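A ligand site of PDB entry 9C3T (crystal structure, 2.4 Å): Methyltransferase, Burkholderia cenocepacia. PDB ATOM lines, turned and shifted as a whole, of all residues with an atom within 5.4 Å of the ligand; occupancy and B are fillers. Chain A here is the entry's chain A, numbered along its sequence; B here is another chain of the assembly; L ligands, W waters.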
ATOM      1  N   ARG A  38     -19.454  12.908   7.336  1.00  0.00           N
ATOM      2  CA  ARG A  38     -20.249  13.824   6.540  1.00  0.00           C
ATOM      3  C   ARG A  38     -19.512  14.179   5.251  1.00  0.00           C
ATOM      4  O   ARG A  38     -18.279  14.166   5.200  1.00  0.00           O
ATOM      5  CB  ARG A  38     -20.575  15.104   7.319  1.00  0.00           C
ATOM      6  N   ASP A  39     -20.290  14.497   4.224  1.00  0.00           N
ATOM      7  CA  ASP A  39     -19.740  15.031   2.989  1.00  0.00           C
ATOM      8  C   ASP A  39     -19.064  16.360   3.287  1.00  0.00           C
ATOM      9  O   ASP A  39     -19.676  17.247   3.892  1.00  0.00           O
ATOM     10  CB  ASP A  39     -20.864  15.196   1.955  1.00  0.00           C
ATOM     11  CG  ASP A  39     -20.419  15.855   0.645  1.00  0.00           C
ATOM     12  OD1 ASP A  39     -19.440  16.624   0.615  1.00  0.00           O
ATOM     13  OD2 ASP A  39     -21.079  15.592  -0.378  1.00  0.00           O
ATOM     14  N   PHE A  40     -17.800  16.489   2.888  1.00  0.00           N
ATOM     15  CA  PHE A  40     -17.049  17.694   3.205  1.00  0.00           C
ATOM     16  C   PHE A  40     -17.626  18.914   2.491  1.00  0.00           C
ATOM     17  O   PHE A  40     -17.626  20.023   3.046  1.00  0.00           O
ATOM     18  CB  PHE A  40     -15.578  17.521   2.848  1.00  0.00           C
ATOM     19  CG  PHE A  40     -14.787  18.803   2.860  1.00  0.00           C
ATOM     20  CD1 PHE A  40     -14.379  19.361   4.058  1.00  0.00           C
ATOM     21  CD2 PHE A  40     -14.479  19.458   1.674  1.00  0.00           C
ATOM     22  CE1 PHE A  40     -13.659  20.553   4.078  1.00  0.00           C
ATOM     23  CE2 PHE A  40     -13.766  20.643   1.692  1.00  0.00           C
ATOM     24  CZ  PHE A  40     -13.357  21.185   2.884  1.00  0.00           C
ATOM     25  N   LEU A  41     -18.086  18.737   1.259  1.00  0.00           N
ATOM     26  CA  LEU A  41     -18.524  19.904   0.459  1.00  0.00           C
ATOM     27  C   LEU A  41     -19.867  20.425   0.973  1.00  0.00           C
ATOM     28  O   LEU A  41     -20.202  21.586   0.682  1.00  0.00           O
ATOM     29  CB  LEU A  41     -18.539  19.498  -1.012  1.00  0.00           C
ATOM     30  CG  LEU A  41     -17.172  19.273  -1.662  1.00  0.00           C
ATOM     31  CD1 LEU A  41     -16.863  17.792  -1.806  1.00  0.00           C
ATOM     32  CD2 LEU A  41     -17.158  19.938  -3.023  1.00  0.00           C
ATOM     33  N   ASP A  58      -5.706  14.113   0.807  1.00  0.00           N
ATOM     34  CA  ASP A  58      -5.505  12.930  -0.025  1.00  0.00           C
ATOM     35  C   ASP A  58      -6.817  12.628  -0.741  1.00  0.00           C
ATOM     36  O   ASP A  58      -7.463  11.603  -0.466  1.00  0.00           O
ATOM     37  CB  ASP A  58      -5.036  11.736   0.805  1.00  0.00           C
ATOM     38  CG  ASP A  58      -4.694  10.532  -0.054  1.00  0.00           C
ATOM     39  OD1 ASP A  58      -4.372  10.717  -1.241  1.00  0.00           O
ATOM     40  OD2 ASP A  58      -4.754   9.401   0.472  1.00  0.00           O
ATOM     41  N   PRO A  59      -7.235  13.482  -1.659  1.00  0.00           N
ATOM     42  CA  PRO A  59      -8.538  13.296  -2.303  1.00  0.00           C
ATOM     43  C   PRO A  59      -8.472  12.188  -3.331  1.00  0.00           C
ATOM     44  O   PRO A  59      -7.381  11.690  -3.640  1.00  0.00           O
ATOM     45  CB  PRO A  59      -8.797  14.661  -2.963  1.00  0.00           C
ATOM     46  CG  PRO A  59      -7.437  15.200  -3.245  1.00  0.00           C
ATOM     47  CD  PRO A  59      -6.455  14.549  -2.303  1.00  0.00           C
ATOM     48  N   PRO A  60      -9.620  11.747  -3.856  1.00  0.00           N
ATOM     49  CA  PRO A  60      -9.594  10.815  -4.980  1.00  0.00           C
ATOM     50  C   PRO A  60      -8.756  11.366  -6.128  1.00  0.00           C
ATOM     51  O   PRO A  60      -8.803  12.550  -6.444  1.00  0.00           O
ATOM     52  CB  PRO A  60     -11.070  10.677  -5.385  1.00  0.00           C
ATOM     53  CG  PRO A  60     -11.843  11.619  -4.492  1.00  0.00           C
ATOM     54  CD  PRO A  60     -10.980  11.925  -3.323  1.00  0.00           C
ATOM     55  N   TYR A  67     -14.372   3.277  -3.432  1.00  0.00           N
ATOM     56  CA  TYR A  67     -14.355   3.674  -2.002  1.00  0.00           C
ATOM     57  C   TYR A  67     -15.720   3.440  -1.416  1.00  0.00           C
ATOM     58  O   TYR A  67     -16.061   4.081  -0.415  1.00  0.00           O
ATOM     59  CB  TYR A  67     -14.016   5.162  -1.903  1.00  0.00           C
ATOM     60  CG  TYR A  67     -12.603   5.613  -2.219  1.00  0.00           C
ATOM     61  CD1 TYR A  67     -11.506   5.003  -1.619  1.00  0.00           C
ATOM     62  CD2 TYR A  67     -12.364   6.676  -3.076  1.00  0.00           C
ATOM     63  CE1 TYR A  67     -10.221   5.426  -1.889  1.00  0.00           C
ATOM     64  CE2 TYR A  67     -11.076   7.112  -3.349  1.00  0.00           C
ATOM     65  CZ  TYR A  67     -10.002   6.483  -2.753  1.00  0.00           C
ATOM     66  OH  TYR A  67      -8.739   6.898  -3.007  1.00  0.00           O
ATOM     67  N   ASN A  69     -18.154   4.183  -3.115  1.00  0.00           N
ATOM     68  CA  ASN A  69     -18.843   5.346  -3.735  1.00  0.00           C
ATOM     69  C   ASN A  69     -18.192   5.613  -5.090  1.00  0.00           C
ATOM     70  O   ASN A  69     -17.355   4.799  -5.526  1.00  0.00           O
ATOM     71  CB  ASN A  69     -18.787   6.569  -2.834  1.00  0.00           C
ATOM     72  CG  ASN A  69     -17.507   6.677  -2.056  1.00  0.00           C
ATOM     73  OD1 ASN A  69     -16.508   7.190  -2.563  1.00  0.00           O
ATOM     74  ND2 ASN A  69     -17.520   6.223  -0.807  1.00  0.00           N
ATOM     75  N   SER A  71     -16.505   8.551  -5.924  1.00  0.00           N
ATOM     76  CA  SER A  71     -15.631   9.738  -5.776  1.00  0.00           C
ATOM     77  C   SER A  71     -14.452   9.644  -6.747  1.00  0.00           C
ATOM     78  O   SER A  71     -14.050  10.684  -7.278  1.00  0.00           O
ATOM     79  CB  SER A  71     -15.174   9.835  -4.367  1.00  0.00           C
ATOM     80  OG  SER A  71     -14.943   8.556  -3.809  1.00  0.00           O
ATOM     81  N   TRP A  82     -14.558  19.210 -10.158  1.00  0.00           N
ATOM     82  CA  TRP A  82     -14.869  18.842  -8.752  1.00  0.00           C
ATOM     83  C   TRP A  82     -13.714  19.207  -7.815  1.00  0.00           C
ATOM     84  O   TRP A  82     -13.990  19.705  -6.717  1.00  0.00           O
ATOM     85  CB  TRP A  82     -15.218  17.356  -8.644  1.00  0.00           C
ATOM     86  CG  TRP A  82     -15.384  16.847  -7.242  1.00  0.00           C
ATOM     87  CD1 TRP A  82     -16.505  16.882  -6.476  1.00  0.00           C
ATOM     88  CD2 TRP A  82     -14.367  16.213  -6.434  1.00  0.00           C
ATOM     89  NE1 TRP A  82     -16.271  16.311  -5.253  1.00  0.00           N
ATOM     90  CE2 TRP A  82     -14.965  15.892  -5.198  1.00  0.00           C
ATOM     91  CE3 TRP A  82     -13.026  15.882  -6.633  1.00  0.00           C
ATOM     92  CZ2 TRP A  82     -14.267  15.264  -4.175  1.00  0.00           C
ATOM     93  CZ3 TRP A  82     -12.334  15.262  -5.615  1.00  0.00           C
ATOM     94  CH2 TRP A  82     -12.957  14.961  -4.406  1.00  0.00           C
ATOM     95  N   HIS A 213      -8.962  -0.364   3.967  1.00  0.00           N
ATOM     96  CA  HIS A 213      -9.177   0.819   3.096  1.00  0.00           C
ATOM     97  C   HIS A 213      -8.302   0.608   1.859  1.00  0.00           C
ATOM     98  O   HIS A 213      -7.134   0.196   1.990  1.00  0.00           O
ATOM     99  CB  HIS A 213      -8.853   2.119   3.828  1.00  0.00           C
ATOM    100  CG  HIS A 213      -9.217   3.358   3.083  1.00  0.00           C
ATOM    101  ND1 HIS A 213      -8.437   3.899   2.093  1.00  0.00           N
ATOM    102  CD2 HIS A 213     -10.277   4.155   3.202  1.00  0.00           C
ATOM    103  CE1 HIS A 213      -9.026   4.975   1.624  1.00  0.00           C
ATOM    104  NE2 HIS A 213     -10.144   5.154   2.275  1.00  0.00           N
ATOM    105  N   THR A 215      -6.887   2.667  -0.387  1.00  0.00           N
ATOM    106  CA  THR A 215      -5.783   3.590  -0.598  1.00  0.00           C
ATOM    107  C   THR A 215      -5.298   4.107   0.742  1.00  0.00           C
ATOM    108  O   THR A 215      -5.436   5.299   0.998  1.00  0.00           O
ATOM    109  CB  THR A 215      -6.260   4.716  -1.512  1.00  0.00           C
ATOM    110  OG1 THR A 215      -7.217   5.486  -0.780  1.00  0.00           O
ATOM    111  CG2 THR A 215      -6.913   4.182  -2.781  1.00  0.00           C
ATOM    112  N   GLN A 216      -4.735   3.229   1.546  1.00  0.00           N
ATOM    113  CA  GLN A 216      -4.172   3.660   2.851  1.00  0.00           C
ATOM    114  C   GLN A 216      -2.775   4.244   2.671  1.00  0.00           C
ATOM    115  O   GLN A 216      -1.925   3.572   2.080  1.00  0.00           O
ATOM    116  CB  GLN A 216      -4.061   2.524   3.867  1.00  0.00           C
ATOM    117  CG  GLN A 216      -3.862   3.017   5.299  1.00  0.00           C
ATOM    118  CD  GLN A 216      -3.822   1.880   6.287  1.00  0.00           C
ATOM    119  OE1 GLN A 216      -4.281   0.775   6.005  1.00  0.00           O
ATOM    120  NE2 GLN A 216      -3.267   2.140   7.469  1.00  0.00           N
ATOM    121  N   LYS A 217      -2.563   5.460   3.159  1.00  0.00           N
ATOM    122  CA  LYS A 217      -1.238   6.096   3.069  1.00  0.00           C
ATOM    123  C   LYS A 217      -0.411   5.711   4.300  1.00  0.00           C
ATOM    124  O   LYS A 217      -0.988   5.537   5.382  1.00  0.00           O
ATOM    125  CB  LYS A 217      -1.445   7.613   2.899  1.00  0.00           C
ATOM    126  CG  LYS A 217      -2.161   8.000   1.623  1.00  0.00           C
ATOM    127  CD  LYS A 217      -1.225   8.161   0.431  1.00  0.00           C
ATOM    128  CE  LYS A 217      -1.952   8.159  -0.866  1.00  0.00           C
ATOM    129  NZ  LYS A 217      -3.120   7.283  -0.826  1.00  0.00           N
ATOM    130  N   ASP A 238      -8.483  17.150   7.316  1.00  0.00           N
ATOM    131  CA  ASP A 238      -8.411  16.162   6.202  1.00  0.00           C
ATOM    132  C   ASP A 238      -9.809  16.148   5.574  1.00  0.00           C
ATOM    133  O   ASP A 238     -10.677  15.429   6.100  1.00  0.00           O
ATOM    134  CB  ASP A 238      -7.955  14.791   6.664  1.00  0.00           C
ATOM    135  CG  ASP A 238      -7.382  13.906   5.578  1.00  0.00           C
ATOM    136  OD1 ASP A 238      -7.701  14.133   4.392  1.00  0.00           O
ATOM    137  OD2 ASP A 238      -6.629  12.975   5.917  1.00  0.00           O
ATOM    138  N   PRO A 239     -10.067  16.922   4.497  1.00  0.00           N
ATOM    139  CA  PRO A 239     -11.368  16.901   3.876  1.00  0.00           C
ATOM    140  C   PRO A 239     -11.810  15.490   3.538  1.00  0.00           C
ATOM    141  O   PRO A 239     -13.012  15.214   3.523  1.00  0.00           O
ATOM    142  CB  PRO A 239     -11.098  17.736   2.648  1.00  0.00           C
ATOM    143  CG  PRO A 239     -10.034  18.703   3.075  1.00  0.00           C
ATOM    144  CD  PRO A 239      -9.111  17.820   3.880  1.00  0.00           C
ATOM    145  N   PHE A 240     -10.863  14.591   3.269  1.00  0.00           N
ATOM    146  CA  PHE A 240     -11.162  13.192   2.885  1.00  0.00           C
ATOM    147  C   PHE A 240     -10.205  12.321   3.666  1.00  0.00           C
ATOM    148  O   PHE A 240      -9.209  11.883   3.081  1.00  0.00           O
ATOM    149  CB  PHE A 240     -11.020  13.110   1.366  1.00  0.00           C
ATOM    150  CG  PHE A 240     -11.519  14.290   0.550  1.00  0.00           C
ATOM    151  CD1 PHE A 240     -12.871  14.434   0.263  1.00  0.00           C
ATOM    152  CD2 PHE A 240     -10.641  15.268   0.080  1.00  0.00           C
ATOM    153  CE1 PHE A 240     -13.325  15.514  -0.475  1.00  0.00           C
ATOM    154  CE2 PHE A 240     -11.106  16.343  -0.650  1.00  0.00           C
ATOM    155  CZ  PHE A 240     -12.449  16.459  -0.926  1.00  0.00           C
ATOM    156  N   MET A 241     -10.511  12.039   4.929  1.00  0.00           N
ATOM    157  CA  MET A 241      -9.568  11.344   5.846  1.00  0.00           C
ATOM    158  C   MET A 241      -9.489   9.824   5.622  1.00  0.00           C
ATOM    159  O   MET A 241      -8.532   9.211   6.134  1.00  0.00           O
ATOM    160  CB  MET A 241      -9.962  11.614   7.302  1.00  0.00           C
ATOM    161  CG  MET A 241     -11.290  11.043   7.706  1.00  0.00           C
ATOM    162  SD  MET A 241     -11.367  10.852   9.502  1.00  0.00           S
ATOM    163  CE  MET A 241     -13.125  10.564   9.714  1.00  0.00           C
ATOM    164  N   GLY A 242     -10.469   9.245   4.946  1.00  0.00           N
ATOM    165  CA  GLY A 242     -10.481   7.800   4.732  1.00  0.00           C
ATOM    166  C   GLY A 242     -10.409   7.018   6.014  1.00  0.00           C
ATOM    167  O   GLY A 242     -11.380   7.064   6.770  1.00  0.00           O
ATOM    168  N   SER A 243      -9.294   6.333   6.264  1.00  0.00           N
ATOM    169  CA  SER A 243      -9.159   5.432   7.448  1.00  0.00           C
ATOM    170  C   SER A 243      -8.565   6.160   8.652  1.00  0.00           C
ATOM    171  O   SER A 243      -8.310   5.497   9.664  1.00  0.00           O
ATOM    172  CB  SER A 243      -8.322   4.246   7.080  1.00  0.00           C
ATOM    173  OG  SER A 243      -6.961   4.623   6.897  1.00  0.00           O
ATOM    174  N   GLY A 244      -8.308   7.457   8.548  1.00  0.00           N
ATOM    175  CA  GLY A 244      -7.839   8.250   9.696  1.00  0.00           C
ATOM    176  C   GLY A 244      -6.362   8.167   9.949  1.00  0.00           C
ATOM    177  O   GLY A 244      -5.981   8.104  11.127  1.00  0.00           O
ATOM    178  N   THR A 245      -5.548   8.194   8.901  1.00  0.00           N
ATOM    179  CA  THR A 245      -4.083   8.175   9.066  1.00  0.00           C
ATOM    180  C   THR A 245      -3.654   9.513   9.606  1.00  0.00           C
ATOM    181  O   THR A 245      -2.778   9.550  10.477  1.00  0.00           O
ATOM    182  CB  THR A 245      -3.400   7.834   7.732  1.00  0.00           C
ATOM    183  OG1 THR A 245      -3.990   6.618   7.305  1.00  0.00           O
ATOM    184  CG2 THR A 245      -1.901   7.657   7.864  1.00  0.00           C
ATOM    185  N   THR A 246      -4.277  10.585   9.126  1.00  0.00           N
ATOM    186  CA  THR A 246      -3.938  11.940   9.571  1.00  0.00           C
ATOM    187  C   THR A 246      -4.432  12.115  10.992  1.00  0.00           C
ATOM    188  O   THR A 246      -3.757  12.819  11.757  1.00  0.00           O
ATOM    189  CB  THR A 246      -4.514  12.961   8.601  1.00  0.00           C
ATOM    190  OG1 THR A 246      -4.440  12.365   7.305  1.00  0.00           O
ATOM    191  CG2 THR A 246      -3.751  14.272   8.628  1.00  0.00           C
ATOM    192  N   TYR A 260     -13.350  14.517   7.504  1.00  0.00           N
ATOM    193  CA  TYR A 260     -14.658  14.172   6.901  1.00  0.00           C
ATOM    194  C   TYR A 260     -14.503  12.920   6.058  1.00  0.00           C
ATOM    195  O   TYR A 260     -13.537  12.817   5.305  1.00  0.00           O
ATOM    196  CB  TYR A 260     -15.122  15.359   6.075  1.00  0.00           C
ATOM    197  CG  TYR A 260     -15.435  16.619   6.875  1.00  0.00           C
ATOM    198  CD1 TYR A 260     -16.707  16.837   7.387  1.00  0.00           C
ATOM    199  CD2 TYR A 260     -14.469  17.588   7.096  1.00  0.00           C
ATOM    200  CE1 TYR A 260     -17.005  17.984   8.113  1.00  0.00           C
ATOM    201  CE2 TYR A 260     -14.751  18.732   7.818  1.00  0.00           C
ATOM    202  CZ  TYR A 260     -16.016  18.926   8.329  1.00  0.00           C
ATOM    203  OH  TYR A 260     -16.292  20.052   9.036  1.00  0.00           O
ATOM    204  N   GLU A 261     -15.425  11.984   6.200  1.00  0.00           N
ATOM    205  CA  GLU A 261     -15.427  10.782   5.337  1.00  0.00           C
ATOM    206  C   GLU A 261     -16.895  10.349   5.104  1.00  0.00           C
ATOM    207  O   GLU A 261     -17.602  10.145   6.088  1.00  0.00           O
ATOM    208  CB  GLU A 261     -14.583   9.669   5.961  1.00  0.00           C
ATOM    209  CG  GLU A 261     -14.835   8.289   5.357  1.00  0.00           C
ATOM    210  CD  GLU A 261     -14.505   8.194   3.883  1.00  0.00           C
ATOM    211  OE1 GLU A 261     -13.308   8.198   3.570  1.00  0.00           O
ATOM    212  OE2 GLU A 261     -15.424   8.137   3.057  1.00  0.00           O
ATOM    213  N   ILE A 262     -17.313  10.220   3.853  1.00  0.00           N
ATOM    214  CA  ILE A 262     -18.708   9.830   3.527  1.00  0.00           C
ATOM    215  C   ILE A 262     -18.940   8.365   3.930  1.00  0.00           C
ATOM    216  O   ILE A 262     -20.035   8.054   4.389  1.00  0.00           O
ATOM    217  CB  ILE A 262     -18.977  10.073   2.035  1.00  0.00           C
ATOM    218  CG1 ILE A 262     -17.951   9.393   1.150  1.00  0.00           C
ATOM    219  CG2 ILE A 262     -19.064  11.567   1.741  1.00  0.00           C
ATOM    220  CD1 ILE A 262     -18.107   9.718  -0.320  1.00  0.00           C
ATOM    221  N   ASN A 263     -17.932   7.514   3.761  1.00  0.00           N
ATOM    222  CA  ASN A 263     -18.086   6.072   4.056  1.00  0.00           C
ATOM    223  C   ASN A 263     -18.136   5.875   5.564  1.00  0.00           C
ATOM    224  O   ASN A 263     -17.328   6.495   6.272  1.00  0.00           O
ATOM    225  CB  ASN A 263     -16.978   5.265   3.394  1.00  0.00           C
ATOM    226  CG  ASN A 263     -17.208   3.764   3.419  1.00  0.00           C
ATOM    227  OD1 ASN A 263     -17.393   3.190   4.488  1.00  0.00           O
ATOM    228  ND2 ASN A 263     -17.164   3.130   2.265  1.00  0.00           N
ATOM    229  N   TYR A 266     -15.299   3.268   6.828  1.00  0.00           N
ATOM    230  CA  TYR A 266     -13.988   3.931   6.925  1.00  0.00           C
ATOM    231  C   TYR A 266     -13.975   4.755   8.194  1.00  0.00           C
ATOM    232  O   TYR A 266     -13.021   4.657   8.965  1.00  0.00           O
ATOM    233  CB  TYR A 266     -13.701   4.765   5.672  1.00  0.00           C
ATOM    234  CG  TYR A 266     -13.566   4.010   4.354  1.00  0.00           C
ATOM    235  CD1 TYR A 266     -13.336   2.645   4.325  1.00  0.00           C
ATOM    236  CD2 TYR A 266     -13.676   4.681   3.142  1.00  0.00           C
ATOM    237  CE1 TYR A 266     -13.215   1.961   3.127  1.00  0.00           C
ATOM    238  CE2 TYR A 266     -13.566   4.011   1.935  1.00  0.00           C
ATOM    239  CZ  TYR A 266     -13.330   2.651   1.930  1.00  0.00           C
ATOM    240  OH  TYR A 266     -13.226   1.981   0.755  1.00  0.00           O
ATOM    241  N   ARG A 273      -8.747   3.100  15.129  1.00  0.00           N
ATOM    242  CA  ARG A 273      -7.302   3.411  15.009  1.00  0.00           C
ATOM    243  C   ARG A 273      -6.922   4.474  16.048  1.00  0.00           C
ATOM    244  O   ARG A 273      -5.829   4.361  16.612  1.00  0.00           O
ATOM    245  CB  ARG A 273      -7.020   3.820  13.568  1.00  0.00           C
ATOM    246  CG  ARG A 273      -7.075   2.678  12.568  1.00  0.00           C
ATOM    247  CD  ARG A 273      -5.803   2.586  11.744  1.00  0.00           C
ATOM    248  NE  ARG A 273      -5.695   3.672  10.762  1.00  0.00           N
ATOM    249  CZ  ARG A 273      -4.545   4.163  10.331  1.00  0.00           C
ATOM    250  NH1 ARG A 273      -3.474   4.071  11.081  1.00  0.00           N
ATOM    251  NH2 ARG A 273      -4.483   4.749   9.155  1.00  0.00           N
ATOM    252  P    DA B   7      -1.892   1.083  -1.926  1.00  0.00           P
ATOM    253  OP1  DA B   7      -0.823   2.138  -1.809  1.00  0.00           O
ATOM    254  OP2  DA B   7      -2.847   1.078  -0.773  1.00  0.00           O
ATOM    255  O5'  DA B   7      -2.773   1.419  -3.221  1.00  0.00           O
ATOM    256  C5'  DA B   7      -2.195   2.255  -4.249  1.00  0.00           C
ATOM    257  C4'  DA B   7      -3.130   2.288  -5.427  1.00  0.00           C
ATOM    258  O4'  DA B   7      -4.235   3.161  -5.114  1.00  0.00           O
ATOM    259  C3'  DA B   7      -2.522   2.855  -6.703  1.00  0.00           C
ATOM    260  O3'  DA B   7      -3.243   2.375  -7.836  1.00  0.00           O
ATOM    261  C2'  DA B   7      -2.752   4.342  -6.508  1.00  0.00           C
ATOM    262  C1'  DA B   7      -4.137   4.348  -5.906  1.00  0.00           C
ATOM    263  N9   DA B   7      -4.417   5.492  -5.039  1.00  0.00           N
ATOM    264  C8   DA B   7      -3.701   5.912  -3.959  1.00  0.00           C
ATOM    265  N7   DA B   7      -4.205   6.973  -3.380  1.00  0.00           N
ATOM    266  C5   DA B   7      -5.335   7.262  -4.140  1.00  0.00           C
ATOM    267  C6   DA B   7      -6.296   8.274  -4.040  1.00  0.00           C
ATOM    268  N6   DA B   7      -6.288   9.219  -3.105  1.00  0.00           N
ATOM    269  N1   DA B   7      -7.286   8.289  -4.958  1.00  0.00           N
ATOM    270  C2   DA B   7      -7.298   7.334  -5.903  1.00  0.00           C
ATOM    271  N3   DA B   7      -6.438   6.335  -6.091  1.00  0.00           N
ATOM    272  C4   DA B   7      -5.477   6.354  -5.171  1.00  0.00           C
HETATM  273  N1  LIG L   1      -5.732   9.260   3.449  1.00  0.00           N
HETATM  274  C1  LIG L   1      -6.821   8.250   3.534  1.00  0.00           C
HETATM  275  C2  LIG L   1      -6.283   7.002   4.228  1.00  0.00           C
HETATM  276  O1  LIG L   1      -7.080   6.086   4.459  1.00  0.00           O
HETATM  277  O2  LIG L   1      -5.098   6.993   4.512  1.00  0.00           O
HETATM  278  C3  LIG L   1      -7.371   7.979   2.135  1.00  0.00           C
HETATM  279  C4  LIG L   1      -8.440   8.935   1.675  1.00  0.00           C
HETATM  280  C5  LIG L   1      -9.035   8.584   0.314  1.00  0.00           C
HETATM  281  N2  LIG L   1      -7.948   8.690  -0.714  1.00  0.00           N
HETATM  282  C6  LIG L   1     -10.195   9.498  -0.027  1.00  0.00           C
HETATM  283  C7  LIG L   1     -11.449   9.261   0.771  1.00  0.00           C
HETATM  284  O3  LIG L   1     -12.323  10.403   0.648  1.00  0.00           O
HETATM  285  C8  LIG L   1     -12.251   8.054   0.301  1.00  0.00           C
HETATM  286  O4  LIG L   1     -12.238   7.051   1.320  1.00  0.00           O
HETATM  287  C9  LIG L   1     -13.660   8.607   0.036  1.00  0.00           C
HETATM  288  O5  LIG L   1     -14.676   7.758   0.528  1.00  0.00           O
HETATM  289  C10 LIG L   1     -13.636   9.933   0.775  1.00  0.00           C
HETATM  290  N3  LIG L   1     -14.516  10.949   0.219  1.00  0.00           N
HETATM  291  C11 LIG L   1     -14.917  11.077  -1.084  1.00  0.00           C
HETATM  292  N4  LIG L   1     -15.698  12.107  -1.284  1.00  0.00           N
HETATM  293  C12 LIG L   1     -15.829  12.686  -0.039  1.00  0.00           C
HETATM  294  C13 LIG L   1     -16.533  13.824   0.406  1.00  0.00           C
HETATM  295  N5  LIG L   1     -17.279  14.587  -0.385  1.00  0.00           N
HETATM  296  N6  LIG L   1     -16.451  14.135   1.719  1.00  0.00           N
HETATM  297  C14 LIG L   1     -15.707  13.358   2.512  1.00  0.00           C
HETATM  298  N7  LIG L   1     -14.997  12.278   2.209  1.00  0.00           N
HETATM  299  C15 LIG L   1     -15.102  11.993   0.902  1.00  0.00           C
HETATM  300  O   HOH W   1     -17.425  12.750  -3.851  1.00  0.00           O
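O of Tyr 260 lies close to N7 of the ligand (3.5 Å).
Arg 38 touches the ligand.
CD1 of Leu 41 touches N5 of the ligand, 3.5 Å away.
Ser 71 touches the ligand.
Gln 216 touches the ligand (CA to O2, 3.8 Å).
Pro 239 touches the ligand (O to C14, 3.4 Å).
Phe 240 touches the ligand.
O of Met 241 touches C1 of the ligand, 3.3 Å away.
C of Gly 242 touches O1 of the ligand (3.8 Å).
N of Ile 262 touches N7 of the ligand (3.5 Å).
Tyr 266 touches the ligand.
Hydrophobic or aromatic side chains within 4 Å of the ligand: Phe 40, Leu 41, Tyr 67, His 213, Phe 240, Ile 262 and Tyr 266.
Of the 31 residues printed, 23 come within 4 Å of the ligand.
N7 of DA 7 of chain B lies within hydrogen-bond range of the side-chain amino group (NZ) of Lys 217 (2.8 Å).
OD2 of Asp 58 is in salt-bridge range of NZ of Lys 217 (3.0 Å).
OG1 of Thr 215 sits at hydrogen-bond distance from OH of Tyr 67 (3.0 Å).
The side-chain amide nitrogen (ND2) of Asn 69 sits at hydrogen-bond distance from the backbone carbonyl oxygen (O) of Tyr 67.
OG1 of Thr 245 sits at hydrogen-bond distance from NH2 of Arg 273.
The backbone NH of Phe 240 sits close to the side-chain carboxylate of Asp 238 (3.4 Å).
The backbone carbonyl oxygen of Tyr 260 sits at hydrogen-bond distance from the backbone NH of Met 241 (3.1 Å).
NE2 of Gln 216 sits close to NH2 of Arg 273 (3.3 Å).
O5 of the ligand sits at hydrogen-bond distance from OE2 of Glu 261 (2.7 Å).
N of Ser 243 lies within hydrogen-bond range of O1 of the ligand (2.9 Å).
O1 of the ligand is in hydrogen-bond range of OG of Ser 243 (2.8 Å).
N6 of the ligand lies within hydrogen-bond range of N of Phe 40 (3.0 Å).
N6 of DA 7 of chain B lies within hydrogen-bond range of a nitrogen (N2) of the ligand (3.0 Å).
A nitrogen (N2) of the ligand is in hydrogen-bond range of the backbone carbonyl oxygen (O) of Asp 58 (3.0 Å).
The side-chain carboxylate (OD2) of Asp 58 is in salt-bridge range of a nitrogen (N1) of the ligand, 3.1 Å away.
A ring nitrogen (NE2) of His 213 is in hydrogen-bond range of an oxygen (O4) of the ligand (3.0 Å).
OH of Tyr 67 is in hydrogen-bond range of N2 of the ligand, 3.0 Å away.
O2 of the ligand sits at hydrogen-bond distance from OG1 of Thr 245 (3.0 Å).
The side-chain carboxylate of Asp 39 lies within hydrogen-bond range of a nitrogen (N5) of the ligand (3.1 Å).
N of Lys 217 is in hydrogen-bond range of O2 of the ligand (3.3 Å).
The side-chain hydroxyl of Thr 215 is in hydrogen-bond range of a nitrogen (N2) of the ligand, 3.3 Å away.
The side-chain amide nitrogen (ND2) of Asn 69 sits at hydrogen-bond distance from an oxygen (O5) of the ligand, 3.5 Å away.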
